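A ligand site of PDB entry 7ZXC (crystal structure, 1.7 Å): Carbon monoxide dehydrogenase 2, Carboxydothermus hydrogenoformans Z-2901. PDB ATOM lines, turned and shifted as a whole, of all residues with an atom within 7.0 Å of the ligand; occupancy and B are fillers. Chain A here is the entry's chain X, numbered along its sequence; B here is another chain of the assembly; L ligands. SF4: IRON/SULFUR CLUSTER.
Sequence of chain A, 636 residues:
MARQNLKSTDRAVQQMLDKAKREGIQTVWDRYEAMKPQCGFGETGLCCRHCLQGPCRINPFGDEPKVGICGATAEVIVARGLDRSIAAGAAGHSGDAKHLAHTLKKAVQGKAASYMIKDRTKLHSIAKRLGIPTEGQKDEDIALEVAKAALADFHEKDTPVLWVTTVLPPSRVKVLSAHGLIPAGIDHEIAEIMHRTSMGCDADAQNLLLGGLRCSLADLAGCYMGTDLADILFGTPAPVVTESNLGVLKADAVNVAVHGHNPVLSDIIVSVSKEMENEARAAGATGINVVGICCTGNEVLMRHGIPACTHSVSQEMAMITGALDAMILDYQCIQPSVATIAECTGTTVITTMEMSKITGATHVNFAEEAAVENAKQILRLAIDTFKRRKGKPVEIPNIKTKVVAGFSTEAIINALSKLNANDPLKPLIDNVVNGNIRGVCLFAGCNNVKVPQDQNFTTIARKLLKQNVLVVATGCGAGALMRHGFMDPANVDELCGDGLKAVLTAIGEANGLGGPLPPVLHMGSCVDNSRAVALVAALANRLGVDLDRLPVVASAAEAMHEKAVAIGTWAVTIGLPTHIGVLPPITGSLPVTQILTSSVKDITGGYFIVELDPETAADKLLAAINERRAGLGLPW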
ATOM      1  N   CYS A  47       0.697   5.502  26.003  1.00  0.00           N
ATOM      2  CA  CYS A  47       1.282   4.183  25.874  1.00  0.00           C
ATOM      3  C   CYS A  47       0.247   3.272  25.242  1.00  0.00           C
ATOM      4  O   CYS A  47      -0.955   3.373  25.563  1.00  0.00           O
ATOM      5  CB  CYS A  47       1.722   3.609  27.231  1.00  0.00           C
ATOM      6  SG  CYS A  47       2.486   1.961  27.084  1.00  0.00           S
ATOM      7  N   CYS A  48       0.706   2.401  24.347  1.00  0.00           N
ATOM      8  CA  CYS A  48      -0.157   1.448  23.669  1.00  0.00           C
ATOM      9  C   CYS A  48       0.522   0.096  23.583  1.00  0.00           C
ATOM     10  O   CYS A  48       1.678  -0.023  23.149  1.00  0.00           O
ATOM     11  CB  CYS A  48      -0.529   1.921  22.250  1.00  0.00           C
ATOM     12  SG  CYS A  48      -1.589   0.744  21.440  1.00  0.00           S
ATOM     13  N   ARG A  49      -0.190  -0.934  24.045  1.00  0.00           N
ATOM     14  CA  ARG A  49       0.237  -2.313  23.946  1.00  0.00           C
ATOM     15  C   ARG A  49      -0.802  -3.133  23.203  1.00  0.00           C
ATOM     16  O   ARG A  49      -1.022  -4.301  23.512  1.00  0.00           O
ATOM     17  CB  ARG A  49       0.507  -2.897  25.336  1.00  0.00           C
ATOM     18  CG  ARG A  49       1.609  -2.153  26.096  1.00  0.00           C
ATOM     19  CD  ARG A  49       1.573  -2.505  27.569  1.00  0.00           C
ATOM     20  NE  ARG A  49       1.826  -3.924  27.733  1.00  0.00           N
ATOM     21  CZ  ARG A  49       1.521  -4.636  28.811  1.00  0.00           C
ATOM     22  NH1 ARG A  49       0.966  -4.077  29.893  1.00  0.00           N
ATOM     23  NH2 ARG A  49       1.786  -5.941  28.799  1.00  0.00           N
ATOM     24  N   HIS A  50      -1.458  -2.529  22.216  1.00  0.00           N
ATOM     25  CA  HIS A  50      -2.560  -3.274  21.612  1.00  0.00           C
ATOM     26  C   HIS A  50      -2.082  -4.257  20.543  1.00  0.00           C
ATOM     27  O   HIS A  50      -2.918  -4.977  19.994  1.00  0.00           O
ATOM     28  CB  HIS A  50      -3.609  -2.307  21.047  1.00  0.00           C
ATOM     29  CG  HIS A  50      -4.382  -1.564  22.105  1.00  0.00           C
ATOM     30  ND1 HIS A  50      -5.605  -0.981  21.877  1.00  0.00           N
ATOM     31  CD2 HIS A  50      -4.087  -1.338  23.413  1.00  0.00           C
ATOM     32  CE1 HIS A  50      -6.023  -0.421  22.995  1.00  0.00           C
ATOM     33  NE2 HIS A  50      -5.142  -0.627  23.945  1.00  0.00           N
ATOM     34  N   CYS A  51      -0.775  -4.356  20.296  1.00  0.00           N
ATOM     35  CA  CYS A  51      -0.295  -5.456  19.456  1.00  0.00           C
ATOM     36  C   CYS A  51       1.143  -5.790  19.835  1.00  0.00           C
ATOM     37  O   CYS A  51       1.785  -5.100  20.617  1.00  0.00           O
ATOM     38  CB  CYS A  51      -0.407  -5.113  17.965  1.00  0.00           C
ATOM     39  SG  CYS A  51       0.934  -4.078  17.257  1.00  0.00           S
ATOM     40  N   LEU A  52       1.651  -6.871  19.232  1.00  0.00           N
ATOM     41  CA  LEU A  52       2.965  -7.354  19.610  1.00  0.00           C
ATOM     42  C   LEU A  52       4.096  -6.617  18.925  1.00  0.00           C
ATOM     43  O   LEU A  52       5.263  -6.947  19.164  1.00  0.00           O
ATOM     44  CB  LEU A  52       3.085  -8.848  19.314  1.00  0.00           C
ATOM     45  CG  LEU A  52       2.072  -9.712  20.061  1.00  0.00           C
ATOM     46  CD1 LEU A  52       2.175 -11.192  19.663  1.00  0.00           C
ATOM     47  CD2 LEU A  52       2.249  -9.499  21.582  1.00  0.00           C
ATOM     48  N   GLN A  53       3.797  -5.665  18.059  1.00  0.00           N
ATOM     49  CA  GLN A  53       4.843  -4.730  17.678  1.00  0.00           C
ATOM     50  C   GLN A  53       5.182  -3.762  18.795  1.00  0.00           C
ATOM     51  O   GLN A  53       6.244  -3.146  18.768  1.00  0.00           O
ATOM     52  CB  GLN A  53       4.452  -3.982  16.414  1.00  0.00           C
ATOM     53  CG  GLN A  53       4.285  -4.914  15.251  1.00  0.00           C
ATOM     54  CD  GLN A  53       4.014  -4.211  13.935  1.00  0.00           C
ATOM     55  OE1 GLN A  53       4.455  -4.670  12.868  1.00  0.00           O
ATOM     56  NE2 GLN A  53       3.263  -3.113  13.987  1.00  0.00           N
ATOM     57  N   GLY A  54       4.291  -3.617  19.794  1.00  0.00           N
ATOM     58  CA  GLY A  54       4.542  -2.724  20.903  1.00  0.00           C
ATOM     59  C   GLY A  54       5.502  -3.342  21.896  1.00  0.00           C
ATOM     60  O   GLY A  54       6.072  -4.420  21.664  1.00  0.00           O
ATOM     61  N   PRO A  55       5.679  -2.686  23.048  1.00  0.00           N
ATOM     62  CA  PRO A  55       4.909  -1.497  23.467  1.00  0.00           C
ATOM     63  C   PRO A  55       5.357  -0.223  22.763  1.00  0.00           C
ATOM     64  O   PRO A  55       6.554  -0.032  22.499  1.00  0.00           O
ATOM     65  CB  PRO A  55       5.176  -1.405  24.965  1.00  0.00           C
ATOM     66  CG  PRO A  55       6.472  -2.096  25.171  1.00  0.00           C
ATOM     67  CD  PRO A  55       6.509  -3.209  24.147  1.00  0.00           C
ATOM     68  N   CYS A  56       4.378   0.629  22.465  1.00  0.00           N
ATOM     69  CA  CYS A  56       4.620   1.935  21.884  1.00  0.00           C
ATOM     70  C   CYS A  56       4.327   3.030  22.898  1.00  0.00           C
ATOM     71  O   CYS A  56       3.440   2.903  23.752  1.00  0.00           O
ATOM     72  CB  CYS A  56       3.723   2.158  20.666  1.00  0.00           C
ATOM     73  SG  CYS A  56       4.130   1.127  19.254  1.00  0.00           S
ATOM     74  N   ARG A  57       5.072   4.110  22.796  1.00  0.00           N
ATOM     75  CA  ARG A  57       4.845   5.259  23.655  1.00  0.00           C
ATOM     76  C   ARG A  57       5.056   6.525  22.831  1.00  0.00           C
ATOM     77  O   ARG A  57       5.633   6.488  21.735  1.00  0.00           O
ATOM     78  CB  ARG A  57       5.784   5.248  24.872  1.00  0.00           C
ATOM     79  CG  ARG A  57       7.215   5.559  24.467  1.00  0.00           C
ATOM     80  CD  ARG A  57       8.232   5.072  25.449  1.00  0.00           C
ATOM     81  NE  ARG A  57       9.544   5.510  24.982  1.00  0.00           N
ATOM     82  CZ  ARG A  57      10.266   4.894  24.058  1.00  0.00           C
ATOM     83  NH1 ARG A  57      11.438   5.420  23.705  1.00  0.00           N
ATOM     84  NH2 ARG A  57       9.849   3.759  23.481  1.00  0.00           N
ATOM     85  N   VAL A  67       4.715   9.163  17.450  1.00  0.00           N
ATOM     86  CA  VAL A  67       3.600   8.442  16.861  1.00  0.00           C
ATOM     87  C   VAL A  67       3.838   6.964  17.112  1.00  0.00           C
ATOM     88  O   VAL A  67       4.987   6.526  17.236  1.00  0.00           O
ATOM     89  CB  VAL A  67       3.507   8.776  15.350  1.00  0.00           C
ATOM     90  CG1 VAL A  67       4.738   8.250  14.615  1.00  0.00           C
ATOM     91  CG2 VAL A  67       2.267   8.185  14.720  1.00  0.00           C
ATOM     92  N   GLY A  68       2.761   6.187  17.220  1.00  0.00           N
ATOM     93  CA  GLY A  68       2.884   4.745  17.364  1.00  0.00           C
ATOM     94  C   GLY A  68       3.430   4.082  16.118  1.00  0.00           C
ATOM     95  O   GLY A  68       3.420   4.637  15.017  1.00  0.00           O
ATOM     96  N   ILE A  69       3.935   2.852  16.286  1.00  0.00           N
ATOM     97  CA  ILE A  69       4.614   2.163  15.191  1.00  0.00           C
ATOM     98  C   ILE A  69       3.684   1.955  14.010  1.00  0.00           C
ATOM     99  O   ILE A  69       4.087   2.079  12.836  1.00  0.00           O
ATOM    100  CB  ILE A  69       5.193   0.829  15.682  1.00  0.00           C
ATOM    101  CG1 ILE A  69       6.441   1.117  16.522  1.00  0.00           C
ATOM    102  CG2 ILE A  69       5.529  -0.112  14.475  1.00  0.00           C
ATOM    103  CD1 ILE A  69       7.048  -0.101  17.161  1.00  0.00           C
ATOM    104  N   CYS A  70       2.411   1.683  14.275  1.00  0.00           N
ATOM    105  CA  CYS A  70       1.479   1.511  13.187  1.00  0.00           C
ATOM    106  C   CYS A  70       1.016   2.831  12.600  1.00  0.00           C
ATOM    107  O   CYS A  70       0.250   2.800  11.640  1.00  0.00           O
ATOM    108  CB  CYS A  70       0.271   0.727  13.654  1.00  0.00           C
ATOM    109  SG  CYS A  70      -0.583   1.575  14.981  1.00  0.00           S
ATOM    110  N   GLY A  71       1.445   3.978  13.151  1.00  0.00           N
ATOM    111  CA  GLY A  71       0.886   5.263  12.773  1.00  0.00           C
ATOM    112  C   GLY A  71      -0.137   5.842  13.720  1.00  0.00           C
ATOM    113  O   GLY A  71      -0.579   6.978  13.502  1.00  0.00           O
ATOM    114  N   ALA A  72      -0.522   5.120  14.776  1.00  0.00           N
ATOM    115  CA  ALA A  72      -1.511   5.647  15.723  1.00  0.00           C
ATOM    116  C   ALA A  72      -1.008   6.930  16.380  1.00  0.00           C
ATOM    117  O   ALA A  72       0.069   6.964  16.977  1.00  0.00           O
ATOM    118  CB  ALA A  72      -1.832   4.613  16.795  1.00  0.00           C
ATOM    119  N   THR A  73      -1.822   7.980  16.308  1.00  0.00           N
ATOM    120  CA  THR A  73      -1.485   9.262  16.917  1.00  0.00           C
ATOM    121  C   THR A  73      -1.715   9.238  18.427  1.00  0.00           C
ATOM    122  O   THR A  73      -2.316   8.321  18.972  1.00  0.00           O
ATOM    123  CB  THR A  73      -2.330  10.390  16.323  1.00  0.00           C
ATOM    124  OG1 THR A  73      -3.724  10.117  16.533  1.00  0.00           O
ATOM    125  CG2 THR A  73      -2.061  10.560  14.804  1.00  0.00           C
ATOM    126  N   ILE A  77      -4.391   6.860  20.428  1.00  0.00           N
ATOM    127  CA  ILE A  77      -3.900   6.039  21.526  1.00  0.00           C
ATOM    128  C   ILE A  77      -4.631   6.389  22.815  1.00  0.00           C
ATOM    129  O   ILE A  77      -5.090   5.509  23.552  1.00  0.00           O
ATOM    130  CB  ILE A  77      -2.376   6.197  21.662  1.00  0.00           C
ATOM    131  CG1 ILE A  77      -1.679   5.514  20.477  1.00  0.00           C
ATOM    132  CG2 ILE A  77      -1.847   5.659  22.997  1.00  0.00           C
ATOM    133  CD1 ILE A  77      -0.171   5.751  20.424  1.00  0.00           C
ATOM    134  N   ARG A  80      -8.320   5.273  22.534  1.00  0.00           N
ATOM    135  CA  ARG A  80      -8.455   3.826  22.547  1.00  0.00           C
ATOM    136  C   ARG A  80      -8.292   3.277  23.956  1.00  0.00           C
ATOM    137  O   ARG A  80      -9.055   2.391  24.368  1.00  0.00           O
ATOM    138  CB  ARG A  80      -7.435   3.179  21.593  1.00  0.00           C
ATOM    139  CG  ARG A  80      -7.865   3.297  20.124  1.00  0.00           C
ATOM    140  CD  ARG A  80      -7.051   2.403  19.175  1.00  0.00           C
ATOM    141  NE  ARG A  80      -5.613   2.453  19.408  1.00  0.00           N
ATOM    142  CZ  ARG A  80      -4.711   2.016  18.529  1.00  0.00           C
ATOM    143  NH1 ARG A  80      -5.130   1.520  17.354  1.00  0.00           N
ATOM    144  NH2 ARG A  80      -3.405   2.096  18.798  1.00  0.00           N
ATOM    145  N   THR A 197     -10.977  -0.793  19.049  1.00  0.00           N
ATOM    146  CA  THR A 197      -9.741  -0.296  19.631  1.00  0.00           C
ATOM    147  C   THR A 197      -8.555  -1.221  19.378  1.00  0.00           C
ATOM    148  O   THR A 197      -7.439  -0.862  19.766  1.00  0.00           O
ATOM    149  CB  THR A 197      -9.900  -0.072  21.142  1.00  0.00           C
ATOM    150  OG1 THR A 197     -10.229  -1.329  21.770  1.00  0.00           O
ATOM    151  CG2 THR A 197     -10.997   1.011  21.436  1.00  0.00           C
ATOM    152  N   SER A 198      -8.772  -2.385  18.752  1.00  0.00           N
ATOM    153  CA  SER A 198      -7.651  -3.244  18.416  1.00  0.00           C
ATOM    154  C   SER A 198      -6.862  -2.655  17.250  1.00  0.00           C
ATOM    155  O   SER A 198      -7.296  -1.700  16.589  1.00  0.00           O
ATOM    156  CB  SER A 198      -8.130  -4.663  18.121  1.00  0.00           C
ATOM    157  OG  SER A 198      -8.841  -4.710  16.891  1.00  0.00           O
ATOM    158  N   MET A 199      -5.664  -3.205  17.016  1.00  0.00           N
ATOM    159  CA  MET A 199      -4.740  -2.597  16.057  1.00  0.00           C
ATOM    160  C   MET A 199      -5.372  -2.494  14.678  1.00  0.00           C
ATOM    161  O   MET A 199      -6.086  -3.392  14.228  1.00  0.00           O
ATOM    162  CB  MET A 199      -3.426  -3.403  16.005  1.00  0.00           C
ATOM    163  CG  MET A 199      -2.355  -2.865  15.021  1.00  0.00           C
ATOM    164  SD  MET A 199      -2.738  -3.408  13.316  1.00  0.00           S
ATOM    165  CE  MET A 199      -1.315  -2.779  12.424  1.00  0.00           C
ATOM    166  N   GLY A 200      -5.096  -1.377  14.007  1.00  0.00           N
ATOM    167  CA  GLY A 200      -5.513  -1.165  12.649  1.00  0.00           C
ATOM    168  C   GLY A 200      -7.006  -1.039  12.426  1.00  0.00           C
ATOM    169  O   GLY A 200      -7.488  -1.381  11.338  1.00  0.00           O
ATOM    170  N   VAL B  28       6.530   2.379   8.421  1.00  0.00           N
ATOM    171  CA  VAL B  28       6.392   1.614   9.647  1.00  0.00           C
ATOM    172  C   VAL B  28       7.768   1.236  10.196  1.00  0.00           C
ATOM    173  O   VAL B  28       7.968   1.188  11.411  1.00  0.00           O
ATOM    174  CB  VAL B  28       5.504   0.372   9.400  1.00  0.00           C
ATOM    175  CG1 VAL B  28       6.121  -0.522   8.285  1.00  0.00           C
ATOM    176  CG2 VAL B  28       5.289  -0.418  10.674  1.00  0.00           C
ATOM    177  N   MET B  35      11.046   4.257  17.920  1.00  0.00           N
ATOM    178  CA  MET B  35      10.492   3.750  19.173  1.00  0.00           C
ATOM    179  C   MET B  35      11.532   3.002  20.004  1.00  0.00           C
ATOM    180  O   MET B  35      11.292   2.729  21.186  1.00  0.00           O
ATOM    181  CB  MET B  35       9.305   2.820  18.864  1.00  0.00           C
ATOM    182  CG  MET B  35       8.379   2.590  20.051  1.00  0.00           C
ATOM    183  SD  MET B  35       7.554   4.076  20.595  1.00  0.00           S
ATOM    184  CE  MET B  35       6.441   4.388  19.223  1.00  0.00           C
ATOM    185  N   GLN B  38      12.427  -0.060  23.174  1.00  0.00           N
ATOM    186  CA  GLN B  38      11.063  -0.130  23.661  1.00  0.00           C
ATOM    187  C   GLN B  38      11.057  -0.483  25.147  1.00  0.00           C
ATOM    188  O   GLN B  38      12.050  -0.956  25.704  1.00  0.00           O
ATOM    189  CB  GLN B  38      10.277  -1.140  22.841  1.00  0.00           C
ATOM    190  CG  GLN B  38      10.064  -0.666  21.406  1.00  0.00           C
ATOM    191  CD  GLN B  38       9.306  -1.683  20.577  1.00  0.00           C
ATOM    192  OE1 GLN B  38       9.874  -2.645  20.074  1.00  0.00           O
ATOM    193  NE2 GLN B  38       7.990  -1.485  20.465  1.00  0.00           N
ATOM    194  N   PRO B 336      -2.905   3.083  10.426  1.00  0.00           N
ATOM    195  CA  PRO B 336      -3.523   4.396  10.207  1.00  0.00           C
ATOM    196  C   PRO B 336      -2.615   5.364   9.478  1.00  0.00           C
ATOM    197  O   PRO B 336      -3.112   6.373   8.949  1.00  0.00           O
ATOM    198  CB  PRO B 336      -3.839   4.904  11.622  1.00  0.00           C
ATOM    199  CG  PRO B 336      -2.980   4.098  12.533  1.00  0.00           C
ATOM    200  CD  PRO B 336      -2.852   2.745  11.870  1.00  0.00           C
ATOM    201  N   MET B 560       1.575 -10.590  15.216  1.00  0.00           N
ATOM    202  CA  MET B 560       1.436  -9.188  15.579  1.00  0.00           C
ATOM    203  C   MET B 560       0.129  -8.904  16.323  1.00  0.00           C
ATOM    204  O   MET B 560       0.146  -8.372  17.436  1.00  0.00           O
ATOM    205  CB  MET B 560       1.514  -8.317  14.312  1.00  0.00           C
ATOM    206  CG  MET B 560       1.387  -6.803  14.551  1.00  0.00           C
ATOM    207  SD  MET B 560      -0.279  -6.152  14.338  1.00  0.00           S
ATOM    208  CE  MET B 560      -0.635  -6.702  12.676  1.00  0.00           C
HETATM  209 FE1  SF4 L   1       2.121   0.217  18.659  1.00  0.00          FE
HETATM  210 FE2  SF4 L   1       0.593  -1.944  18.067  1.00  0.00          FE
HETATM  211 FE3  SF4 L   1      -0.409   0.080  19.633  1.00  0.00          FE
HETATM  212 FE4  SF4 L   1       0.018   0.545  16.909  1.00  0.00          FE
HETATM  213  S1  SF4 L   1      -1.456  -0.925  17.914  1.00  0.00           S
HETATM  214  S2  SF4 L   1       0.475   1.910  18.634  1.00  0.00           S
HETATM  215  S3  SF4 L   1       1.883  -0.724  16.664  1.00  0.00           S
HETATM  216  S4  SF4 L   1       1.343  -1.349  20.177  1.00  0.00           S
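The backbone NH (N) of His 50 sits close to a sulfur (S4) of the ligand, at 3.7 Å. FE2 of the ligand is bound by SG of Cys 51, at 2.3 Å. A sulfur (S4) of the ligand lies close to the backbone NH of Gly 54 (3.7 Å). S4 of the ligand lies close to N of Cys 51 (3.7 Å). NH2 of Arg 80 sits close to S1 of the ligand (3.7 Å). An iron atom (FE3) of the ligand is bound by the side-chain sulfur (SG) of Cys 48 (2.3 Å). The backbone NH of Cys 70 sits close to a sulfur (S3) of the ligand (3.4 Å). The side-chain sulfur of Cys 56 is bound to an iron atom (FE1) of the ligand (2.3 Å). SG of Cys 70 is bound to FE4 of the ligand (2.3 Å).
Merely in contact with the ligand: Gln 53 (3.8 Å), Gly 68 (3.9 Å), Ile 69 (3.8 Å) and Met 199 (3.6 Å). Hydrophobic or aromatic side chains that line the ligand: Ile 69 and Met 199. Of the 29 residues printed, 11 come within 4 Å of the ligand.
The side-chain sulfur (SG) of Cys 70 lies close to the backbone NH (N) of Ala 72 (3.6 Å). SG of Cys 47 sits close to O of Cys 56 (3.6 Å). SG of Cys 56 sits close to N of Ile 69 (3.4 Å). The backbone carbonyl oxygen (O) of Gln 53 lies within hydrogen-bond range of the side-chain amide nitrogen (NE2) of Gln 38 of chain B (2.9 Å). The backbone NH of Gln 53 sits close to the side-chain sulfur of Cys 51 (3.4 Å). SG of Cys 48 sits close to NH2 of Arg 80. The backbone carbonyl oxygen (O) of Cys 56 lies within hydrogen-bond range of the backbone NH (N) of Cys 48. The side-chain sulfur (SG) of Cys 51 lies close to the side-chain sulfur (SD) of Met 560 of chain B (3.8 Å).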
